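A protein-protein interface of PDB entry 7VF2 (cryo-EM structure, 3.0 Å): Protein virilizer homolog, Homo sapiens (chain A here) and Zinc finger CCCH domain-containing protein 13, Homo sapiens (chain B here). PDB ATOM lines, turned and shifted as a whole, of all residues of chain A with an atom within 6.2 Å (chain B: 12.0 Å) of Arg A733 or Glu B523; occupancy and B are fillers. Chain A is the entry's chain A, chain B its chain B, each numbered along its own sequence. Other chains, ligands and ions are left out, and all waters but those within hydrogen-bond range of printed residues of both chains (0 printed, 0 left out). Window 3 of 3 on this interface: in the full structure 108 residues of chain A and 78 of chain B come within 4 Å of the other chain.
The side-chain carboxylate (OD2) of Asp B521 lies within salt-bridge range of the guanidinium group (NH2) of Arg A733 (3.6 Å).
The guanidinium group of Arg A733 is in salt-bridge range of the side-chain carboxylate of Glu B523 (3.2 Å).
OD1 of Asp B521 sits close to N of Glu B523, at 3.5 Å.
O of Arg A733 sits at hydrogen-bond distance from SG of Cys A736, at 3.1 Å.
Leu A730 touches Leu B524.
CD1 of Leu A730 touches O of Leu B527 (3.7 Å).
N of Ser B528 touches CD1 of Leu A730, at 3.998 Å.
Leu A730 touches Leu B531 (CD1 to CD2, 3.6 Å).
Leu B524 touches Arg A733 (CB to NH2, 3.9 Å).
Arg A733 touches Leu B527.
Leu B524 touches Ala A734 (CD2 to CA, 3.8 Å).
His A737 touches Met B519.
CD2 of Leu B524 touches CD2 of His A737, 3.4 Å away.
CB of Pro B518 touches CE1 of Phe A738 (3.6 Å).
Of chain B, only Asp B521, Glu B523, Leu B524 and Leu B527 come within 4 Å of Arg A733.
Glu B523 touches just one residue of chain A: Arg A733 (3.2 Å).
No residue of chain B comes within 4 Å of Leu A731.
Ala A734 touches just one residue of chain B: Leu B524.
Printed residues of chain B within 4 Å of Leu A730: Leu B524 (3.8 Å), Leu B527 (3.7 Å), Ser B528 (3.998 Å) and Leu B531 (3.6 Å).
Printed residues of chain A within 4 Å of Leu B524: Leu A730 (3.8 Å), Arg A733 (3.9 Å), Ala A734 (3.8 Å) and His A737 (3.4 Å).
Of the printed residues of chain A, Met B519 touches His A737 (3.4 Å).
Printed residues of chain A within 4 Å of Asp B521: Arg A733.
The nearest residue of chain B that does not touch Arg A733 is Leu B525 (6.5 Å).
Of the 16 printed residues of chain B, 8 touch a printed residue of chain A.
Hydrophobic or aromatic side chains of chain B that line the printed part of chain A: Pro B518, Met B519, Leu B524, Leu B527 and Leu B531.
Hydrophobic or aromatic side chains of chain A within 4 Å of the printed part of chain B: Leu A730, Ala A734, His A737 and Phe A738.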
ATOM      1  N   THR A 728       8.805  18.000  29.917  1.00  0.00           N
ATOM      2  CA  THR A 728       8.686  18.127  28.469  1.00  0.00           C
ATOM      3  C   THR A 728       8.889  19.567  28.019  1.00  0.00           C
ATOM      4  O   THR A 728       9.508  19.808  26.983  1.00  0.00           O
ATOM      5  CB  THR A 728       7.335  17.614  27.989  1.00  0.00           C
ATOM      6  OG1 THR A 728       7.050  16.365  28.623  1.00  0.00           O
ATOM      7  CG2 THR A 728       7.366  17.408  26.490  1.00  0.00           C
ATOM      8  N   ASN A 729       8.365  20.537  28.772  1.00  0.00           N
ATOM      9  CA  ASN A 729       8.644  21.933  28.455  1.00  0.00           C
ATOM     10  C   ASN A 729      10.140  22.213  28.489  1.00  0.00           C
ATOM     11  O   ASN A 729      10.704  22.776  27.536  1.00  0.00           O
ATOM     12  CB  ASN A 729       7.913  22.852  29.430  1.00  0.00           C
ATOM     13  CG  ASN A 729       6.417  22.713  29.342  1.00  0.00           C
ATOM     14  OD1 ASN A 729       5.884  22.276  28.326  1.00  0.00           O
ATOM     15  ND2 ASN A 729       5.726  23.081  30.412  1.00  0.00           N
ATOM     16  N   LEU A 730      10.802  21.827  29.580  1.00  0.00           N
ATOM     17  CA  LEU A 730      12.234  22.090  29.676  1.00  0.00           C
ATOM     18  C   LEU A 730      13.009  21.320  28.612  1.00  0.00           C
ATOM     19  O   LEU A 730      14.035  21.800  28.118  1.00  0.00           O
ATOM     20  CB  LEU A 730      12.740  21.758  31.076  1.00  0.00           C
ATOM     21  CG  LEU A 730      12.128  22.642  32.160  1.00  0.00           C
ATOM     22  CD1 LEU A 730      12.694  22.297  33.518  1.00  0.00           C
ATOM     23  CD2 LEU A 730      12.363  24.104  31.839  1.00  0.00           C
ATOM     24  N   LEU A 731      12.514  20.147  28.216  1.00  0.00           N
ATOM     25  CA  LEU A 731      13.183  19.374  27.179  1.00  0.00           C
ATOM     26  C   LEU A 731      13.015  20.025  25.813  1.00  0.00           C
ATOM     27  O   LEU A 731      13.943  20.024  24.999  1.00  0.00           O
ATOM     28  CB  LEU A 731      12.634  17.951  27.175  1.00  0.00           C
ATOM     29  CG  LEU A 731      12.979  17.064  25.987  1.00  0.00           C
ATOM     30  CD1 LEU A 731      14.472  16.858  25.919  1.00  0.00           C
ATOM     31  CD2 LEU A 731      12.256  15.745  26.120  1.00  0.00           C
ATOM     32  N   ILE A 732      11.841  20.601  25.547  1.00  0.00           N
ATOM     33  CA  ILE A 732      11.640  21.343  24.306  1.00  0.00           C
ATOM     34  C   ILE A 732      12.586  22.533  24.249  1.00  0.00           C
ATOM     35  O   ILE A 732      13.179  22.827  23.206  1.00  0.00           O
ATOM     36  CB  ILE A 732      10.172  21.782  24.166  1.00  0.00           C
ATOM     37  CG1 ILE A 732       9.259  20.567  24.037  1.00  0.00           C
ATOM     38  CG2 ILE A 732      10.000  22.689  22.969  1.00  0.00           C
ATOM     39  CD1 ILE A 732       9.654  19.641  22.932  1.00  0.00           C
ATOM     40  N   ARG A 733      12.750  23.231  25.374  1.00  0.00           N
ATOM     41  CA  ARG A 733      13.683  24.358  25.395  1.00  0.00           C
ATOM     42  C   ARG A 733      15.116  23.893  25.145  1.00  0.00           C
ATOM     43  O   ARG A 733      15.844  24.475  24.326  1.00  0.00           O
ATOM     44  CB  ARG A 733      13.581  25.104  26.722  1.00  0.00           C
ATOM     45  CG  ARG A 733      12.256  25.807  26.929  1.00  0.00           C
ATOM     46  CD  ARG A 733      12.267  26.611  28.214  1.00  0.00           C
ATOM     47  NE  ARG A 733      13.479  27.414  28.328  1.00  0.00           N
ATOM     48  CZ  ARG A 733      13.782  28.158  29.385  1.00  0.00           C
ATOM     49  NH1 ARG A 733      12.961  28.202  30.423  1.00  0.00           N
ATOM     50  NH2 ARG A 733      14.907  28.858  29.404  1.00  0.00           N
ATOM     51  N   ALA A 734      15.541  22.844  25.854  1.00  0.00           N
ATOM     52  CA  ALA A 734      16.905  22.352  25.706  1.00  0.00           C
ATOM     53  C   ALA A 734      17.157  21.792  24.316  1.00  0.00           C
ATOM     54  O   ALA A 734      18.306  21.748  23.866  1.00  0.00           O
ATOM     55  CB  ALA A 734      17.199  21.291  26.763  1.00  0.00           C
ATOM     56  N   LEU A 735      16.108  21.347  23.626  1.00  0.00           N
ATOM     57  CA  LEU A 735      16.285  20.850  22.268  1.00  0.00           C
ATOM     58  C   LEU A 735      16.293  21.995  21.264  1.00  0.00           C
ATOM     59  O   LEU A 735      17.004  21.943  20.255  1.00  0.00           O
ATOM     60  CB  LEU A 735      15.186  19.845  21.933  1.00  0.00           C
ATOM     61  CG  LEU A 735      15.500  18.382  22.233  1.00  0.00           C
ATOM     62  CD1 LEU A 735      14.243  17.546  22.119  1.00  0.00           C
ATOM     63  CD2 LEU A 735      16.573  17.861  21.298  1.00  0.00           C
ATOM     64  N   CYS A 736      15.506  23.041  21.523  1.00  0.00           N
ATOM     65  CA  CYS A 736      15.460  24.165  20.596  1.00  0.00           C
ATOM     66  C   CYS A 736      16.743  24.983  20.649  1.00  0.00           C
ATOM     67  O   CYS A 736      17.117  25.603  19.647  1.00  0.00           O
ATOM     68  CB  CYS A 736      14.248  25.052  20.882  1.00  0.00           C
ATOM     69  SG  CYS A 736      14.481  26.266  22.195  1.00  0.00           S
ATOM     70  N   HIS A 737      17.414  25.019  21.804  1.00  0.00           N
ATOM     71  CA  HIS A 737      18.711  25.695  21.853  1.00  0.00           C
ATOM     72  C   HIS A 737      19.695  25.091  20.854  1.00  0.00           C
ATOM     73  O   HIS A 737      20.418  25.825  20.161  1.00  0.00           O
ATOM     74  CB  HIS A 737      19.294  25.631  23.263  1.00  0.00           C
ATOM     75  CG  HIS A 737      18.601  26.524  24.243  1.00  0.00           C
ATOM     76  ND1 HIS A 737      18.432  27.875  24.029  1.00  0.00           N
ATOM     77  CD2 HIS A 737      18.038  26.258  25.444  1.00  0.00           C
ATOM     78  CE1 HIS A 737      17.793  28.404  25.058  1.00  0.00           C
ATOM     79  NE2 HIS A 737      17.539  27.444  25.929  1.00  0.00           N
ATOM     80  N   PHE A 738      19.728  23.760  20.764  1.00  0.00           N
ATOM     81  CA  PHE A 738      20.598  23.089  19.806  1.00  0.00           C
ATOM     82  C   PHE A 738      20.248  23.489  18.380  1.00  0.00           C
ATOM     83  O   PHE A 738      21.130  23.797  17.573  1.00  0.00           O
ATOM     84  CB  PHE A 738      20.493  21.572  19.969  1.00  0.00           C
ATOM     85  CG  PHE A 738      21.261  21.027  21.134  1.00  0.00           C
ATOM     86  CD1 PHE A 738      20.969  21.423  22.424  1.00  0.00           C
ATOM     87  CD2 PHE A 738      22.274  20.108  20.935  1.00  0.00           C
ATOM     88  CE1 PHE A 738      21.671  20.916  23.493  1.00  0.00           C
ATOM     89  CE2 PHE A 738      22.982  19.597  22.000  1.00  0.00           C
ATOM     90  CZ  PHE A 738      22.679  20.002  23.280  1.00  0.00           C
ATOM     91  N   ALA B 517      28.562  23.668  20.142  1.00  0.00           N
ATOM     92  CA  ALA B 517      27.996  23.605  21.480  1.00  0.00           C
ATOM     93  C   ALA B 517      26.730  24.442  21.501  1.00  0.00           C
ATOM     94  O   ALA B 517      26.632  25.429  20.762  1.00  0.00           O
ATOM     95  CB  ALA B 517      28.989  24.111  22.537  1.00  0.00           C
ATOM     96  N   PRO B 518      25.751  24.082  22.323  1.00  0.00           N
ATOM     97  CA  PRO B 518      24.505  24.849  22.375  1.00  0.00           C
ATOM     98  C   PRO B 518      24.690  26.173  23.104  1.00  0.00           C
ATOM     99  O   PRO B 518      25.720  26.446  23.721  1.00  0.00           O
ATOM    100  CB  PRO B 518      23.556  23.925  23.145  1.00  0.00           C
ATOM    101  CG  PRO B 518      24.458  23.125  24.014  1.00  0.00           C
ATOM    102  CD  PRO B 518      25.702  22.896  23.193  1.00  0.00           C
ATOM    103  N   MET B 519      23.652  26.998  23.018  1.00  0.00           N
ATOM    104  CA  MET B 519      23.626  28.292  23.684  1.00  0.00           C
ATOM    105  C   MET B 519      23.393  28.039  25.166  1.00  0.00           C
ATOM    106  O   MET B 519      22.277  27.704  25.578  1.00  0.00           O
ATOM    107  CB  MET B 519      22.542  29.188  23.091  1.00  0.00           C
ATOM    108  CG  MET B 519      22.507  30.587  23.694  1.00  0.00           C
ATOM    109  SD  MET B 519      21.247  31.639  22.956  1.00  0.00           S
ATOM    110  CE  MET B 519      19.767  30.933  23.654  1.00  0.00           C
ATOM    111  N   VAL B 520      24.444  28.177  25.961  1.00  0.00           N
ATOM    112  CA  VAL B 520      24.380  27.853  27.377  1.00  0.00           C
ATOM    113  C   VAL B 520      23.517  28.893  28.071  1.00  0.00           C
ATOM    114  O   VAL B 520      23.951  30.029  28.303  1.00  0.00           O
ATOM    115  CB  VAL B 520      25.786  27.797  27.992  1.00  0.00           C
ATOM    116  CG1 VAL B 520      25.700  27.517  29.482  1.00  0.00           C
ATOM    117  CG2 VAL B 520      26.623  26.744  27.289  1.00  0.00           C
ATOM    118  N   ASP B 521      22.289  28.506  28.393  1.00  0.00           N
ATOM    119  CA  ASP B 521      21.354  29.346  29.125  1.00  0.00           C
ATOM    120  C   ASP B 521      21.253  28.794  30.539  1.00  0.00           C
ATOM    121  O   ASP B 521      20.431  27.911  30.804  1.00  0.00           O
ATOM    122  CB  ASP B 521      19.986  29.369  28.444  1.00  0.00           C
ATOM    123  CG  ASP B 521      19.074  30.448  28.999  1.00  0.00           C
ATOM    124  OD1 ASP B 521      19.496  31.166  29.932  1.00  0.00           O
ATOM    125  OD2 ASP B 521      17.935  30.581  28.498  1.00  0.00           O
ATOM    126  N   ASN B 522      22.094  29.311  31.437  1.00  0.00           N
ATOM    127  CA  ASN B 522      22.171  28.760  32.786  1.00  0.00           C
ATOM    128  C   ASN B 522      20.856  28.907  33.537  1.00  0.00           C
ATOM    129  O   ASN B 522      20.662  28.258  34.568  1.00  0.00           O
ATOM    130  CB  ASN B 522      23.314  29.413  33.558  1.00  0.00           C
ATOM    131  CG  ASN B 522      24.672  29.044  33.001  1.00  0.00           C
ATOM    132  OD1 ASN B 522      25.398  29.891  32.483  1.00  0.00           O
ATOM    133  ND2 ASN B 522      25.026  27.770  33.110  1.00  0.00           N
ATOM    134  N   GLU B 523      19.942  29.745  33.044  1.00  0.00           N
ATOM    135  CA  GLU B 523      18.584  29.727  33.575  1.00  0.00           C
ATOM    136  C   GLU B 523      17.907  28.395  33.281  1.00  0.00           C
ATOM    137  O   GLU B 523      17.270  27.802  34.163  1.00  0.00           O
ATOM    138  CB  GLU B 523      17.775  30.880  32.988  1.00  0.00           C
ATOM    139  CG  GLU B 523      16.276  30.736  33.174  1.00  0.00           C
ATOM    140  CD  GLU B 523      15.485  31.569  32.187  1.00  0.00           C
ATOM    141  OE1 GLU B 523      15.904  32.710  31.899  1.00  0.00           O
ATOM    142  OE2 GLU B 523      14.441  31.084  31.702  1.00  0.00           O
ATOM    143  N   LEU B 524      18.046  27.904  32.049  1.00  0.00           N
ATOM    144  CA  LEU B 524      17.514  26.591  31.705  1.00  0.00           C
ATOM    145  C   LEU B 524      18.186  25.501  32.525  1.00  0.00           C
ATOM    146  O   LEU B 524      17.532  24.553  32.970  1.00  0.00           O
ATOM    147  CB  LEU B 524      17.697  26.323  30.212  1.00  0.00           C
ATOM    148  CG  LEU B 524      17.654  24.851  29.796  1.00  0.00           C
ATOM    149  CD1 LEU B 524      16.231  24.325  29.839  1.00  0.00           C
ATOM    150  CD2 LEU B 524      18.265  24.654  28.423  1.00  0.00           C
ATOM    151  N   LEU B 525      19.498  25.616  32.732  1.00  0.00           N
ATOM    152  CA  LEU B 525      20.216  24.617  33.516  1.00  0.00           C
ATOM    153  C   LEU B 525      19.745  24.615  34.966  1.00  0.00           C
ATOM    154  O   LEU B 525      19.572  23.553  35.573  1.00  0.00           O
ATOM    155  CB  LEU B 525      21.719  24.872  33.437  1.00  0.00           C
ATOM    156  CG  LEU B 525      22.583  23.955  34.298  1.00  0.00           C
ATOM    157  CD1 LEU B 525      22.329  22.515  33.922  1.00  0.00           C
ATOM    158  CD2 LEU B 525      24.049  24.302  34.130  1.00  0.00           C
ATOM    159  N   ARG B 526      19.534  25.802  35.536  1.00  0.00           N
ATOM    160  CA  ARG B 526      19.019  25.890  36.898  1.00  0.00           C
ATOM    161  C   ARG B 526      17.626  25.285  36.992  1.00  0.00           C
ATOM    162  O   ARG B 526      17.321  24.548  37.936  1.00  0.00           O
ATOM    163  CB  ARG B 526      19.006  27.347  37.359  1.00  0.00           C
ATOM    164  CG  ARG B 526      18.437  27.548  38.751  1.00  0.00           C
ATOM    165  CD  ARG B 526      18.195  29.017  39.040  1.00  0.00           C
ATOM    166  NE  ARG B 526      17.526  29.684  37.927  1.00  0.00           N
ATOM    167  CZ  ARG B 526      16.212  29.679  37.734  1.00  0.00           C
ATOM    168  NH1 ARG B 526      15.418  29.041  38.584  1.00  0.00           N
ATOM    169  NH2 ARG B 526      15.690  30.312  36.693  1.00  0.00           N
ATOM    170  N   LEU B 527      16.765  25.585  36.017  1.00  0.00           N
ATOM    171  CA  LEU B 527      15.422  25.013  36.020  1.00  0.00           C
ATOM    172  C   LEU B 527      15.472  23.494  35.907  1.00  0.00           C
ATOM    173  O   LEU B 527      14.746  22.786  36.614  1.00  0.00           O
ATOM    174  CB  LEU B 527      14.594  25.606  34.882  1.00  0.00           C
ATOM    175  CG  LEU B 527      13.836  26.895  35.189  1.00  0.00           C
ATOM    176  CD1 LEU B 527      12.987  27.307  34.000  1.00  0.00           C
ATOM    177  CD2 LEU B 527      12.977  26.725  36.427  1.00  0.00           C
ATOM    178  N   SER B 528      16.333  22.979  35.028  1.00  0.00           N
ATOM    179  CA  SER B 528      16.455  21.538  34.849  1.00  0.00           C
ATOM    180  C   SER B 528      16.943  20.865  36.123  1.00  0.00           C
ATOM    181  O   SER B 528      16.399  19.838  36.542  1.00  0.00           O
ATOM    182  CB  SER B 528      17.400  21.240  33.686  1.00  0.00           C
ATOM    183  OG  SER B 528      17.798  19.882  33.690  1.00  0.00           O
ATOM    184  N   LEU B 529      17.979  21.427  36.749  1.00  0.00           N
ATOM    185  CA  LEU B 529      18.509  20.845  37.977  1.00  0.00           C
ATOM    186  C   LEU B 529      17.473  20.884  39.092  1.00  0.00           C
ATOM    187  O   LEU B 529      17.299  19.906  39.827  1.00  0.00           O
ATOM    188  CB  LEU B 529      19.782  21.576  38.396  1.00  0.00           C
ATOM    189  CG  LEU B 529      21.081  21.023  37.820  1.00  0.00           C
ATOM    190  CD1 LEU B 529      22.249  21.916  38.184  1.00  0.00           C
ATOM    191  CD2 LEU B 529      21.307  19.617  38.327  1.00  0.00           C
ATOM    192  N   ARG B 530      16.773  22.012  39.233  1.00  0.00           N
ATOM    193  CA  ARG B 530      15.748  22.113  40.264  1.00  0.00           C
ATOM    194  C   ARG B 530      14.642  21.093  40.040  1.00  0.00           C
ATOM    195  O   ARG B 530      14.202  20.429  40.984  1.00  0.00           O
ATOM    196  CB  ARG B 530      15.177  23.529  40.296  1.00  0.00           C
ATOM    197  CG  ARG B 530      14.367  23.842  41.541  1.00  0.00           C
ATOM    198  CD  ARG B 530      13.247  24.813  41.224  1.00  0.00           C
ATOM    199  NE  ARG B 530      12.343  24.274  40.214  1.00  0.00           N
ATOM    200  CZ  ARG B 530      11.584  25.019  39.418  1.00  0.00           C
ATOM    201  NH1 ARG B 530      11.618  26.341  39.511  1.00  0.00           N
ATOM    202  NH2 ARG B 530      10.793  24.440  38.525  1.00  0.00           N
ATOM    203  N   LEU B 531      14.197  20.935  38.791  1.00  0.00           N
ATOM    204  CA  LEU B 531      13.136  19.978  38.495  1.00  0.00           C
ATOM    205  C   LEU B 531      13.593  18.549  38.760  1.00  0.00           C
ATOM    206  O   LEU B 531      12.863  17.752  39.360  1.00  0.00           O
ATOM    207  CB  LEU B 531      12.683  20.133  37.045  1.00  0.00           C
ATOM    208  CG  LEU B 531      11.559  19.202  36.600  1.00  0.00           C
ATOM    209  CD1 LEU B 531      10.282  19.488  37.370  1.00  0.00           C
ATOM    210  CD2 LEU B 531      11.330  19.330  35.111  1.00  0.00           C
ATOM    211  N   PHE B 532      14.804  18.209  38.312  1.00  0.00           N
ATOM    212  CA  PHE B 532      15.325  16.861  38.515  1.00  0.00           C
ATOM    213  C   PHE B 532      15.474  16.539  39.995  1.00  0.00           C
ATOM    214  O   PHE B 532      15.109  15.445  40.437  1.00  0.00           O
ATOM    215  CB  PHE B 532      16.657  16.709  37.784  1.00  0.00           C
ATOM    216  CG  PHE B 532      17.324  15.389  38.001  1.00  0.00           C
ATOM    217  CD1 PHE B 532      16.961  14.284  37.256  1.00  0.00           C
ATOM    218  CD2 PHE B 532      18.344  15.260  38.925  1.00  0.00           C
ATOM    219  CE1 PHE B 532      17.584  13.077  37.446  1.00  0.00           C
ATOM    220  CE2 PHE B 532      18.967  14.048  39.117  1.00  0.00           C
ATOM    221  CZ  PHE B 532      18.587  12.951  38.376  1.00  0.00           C
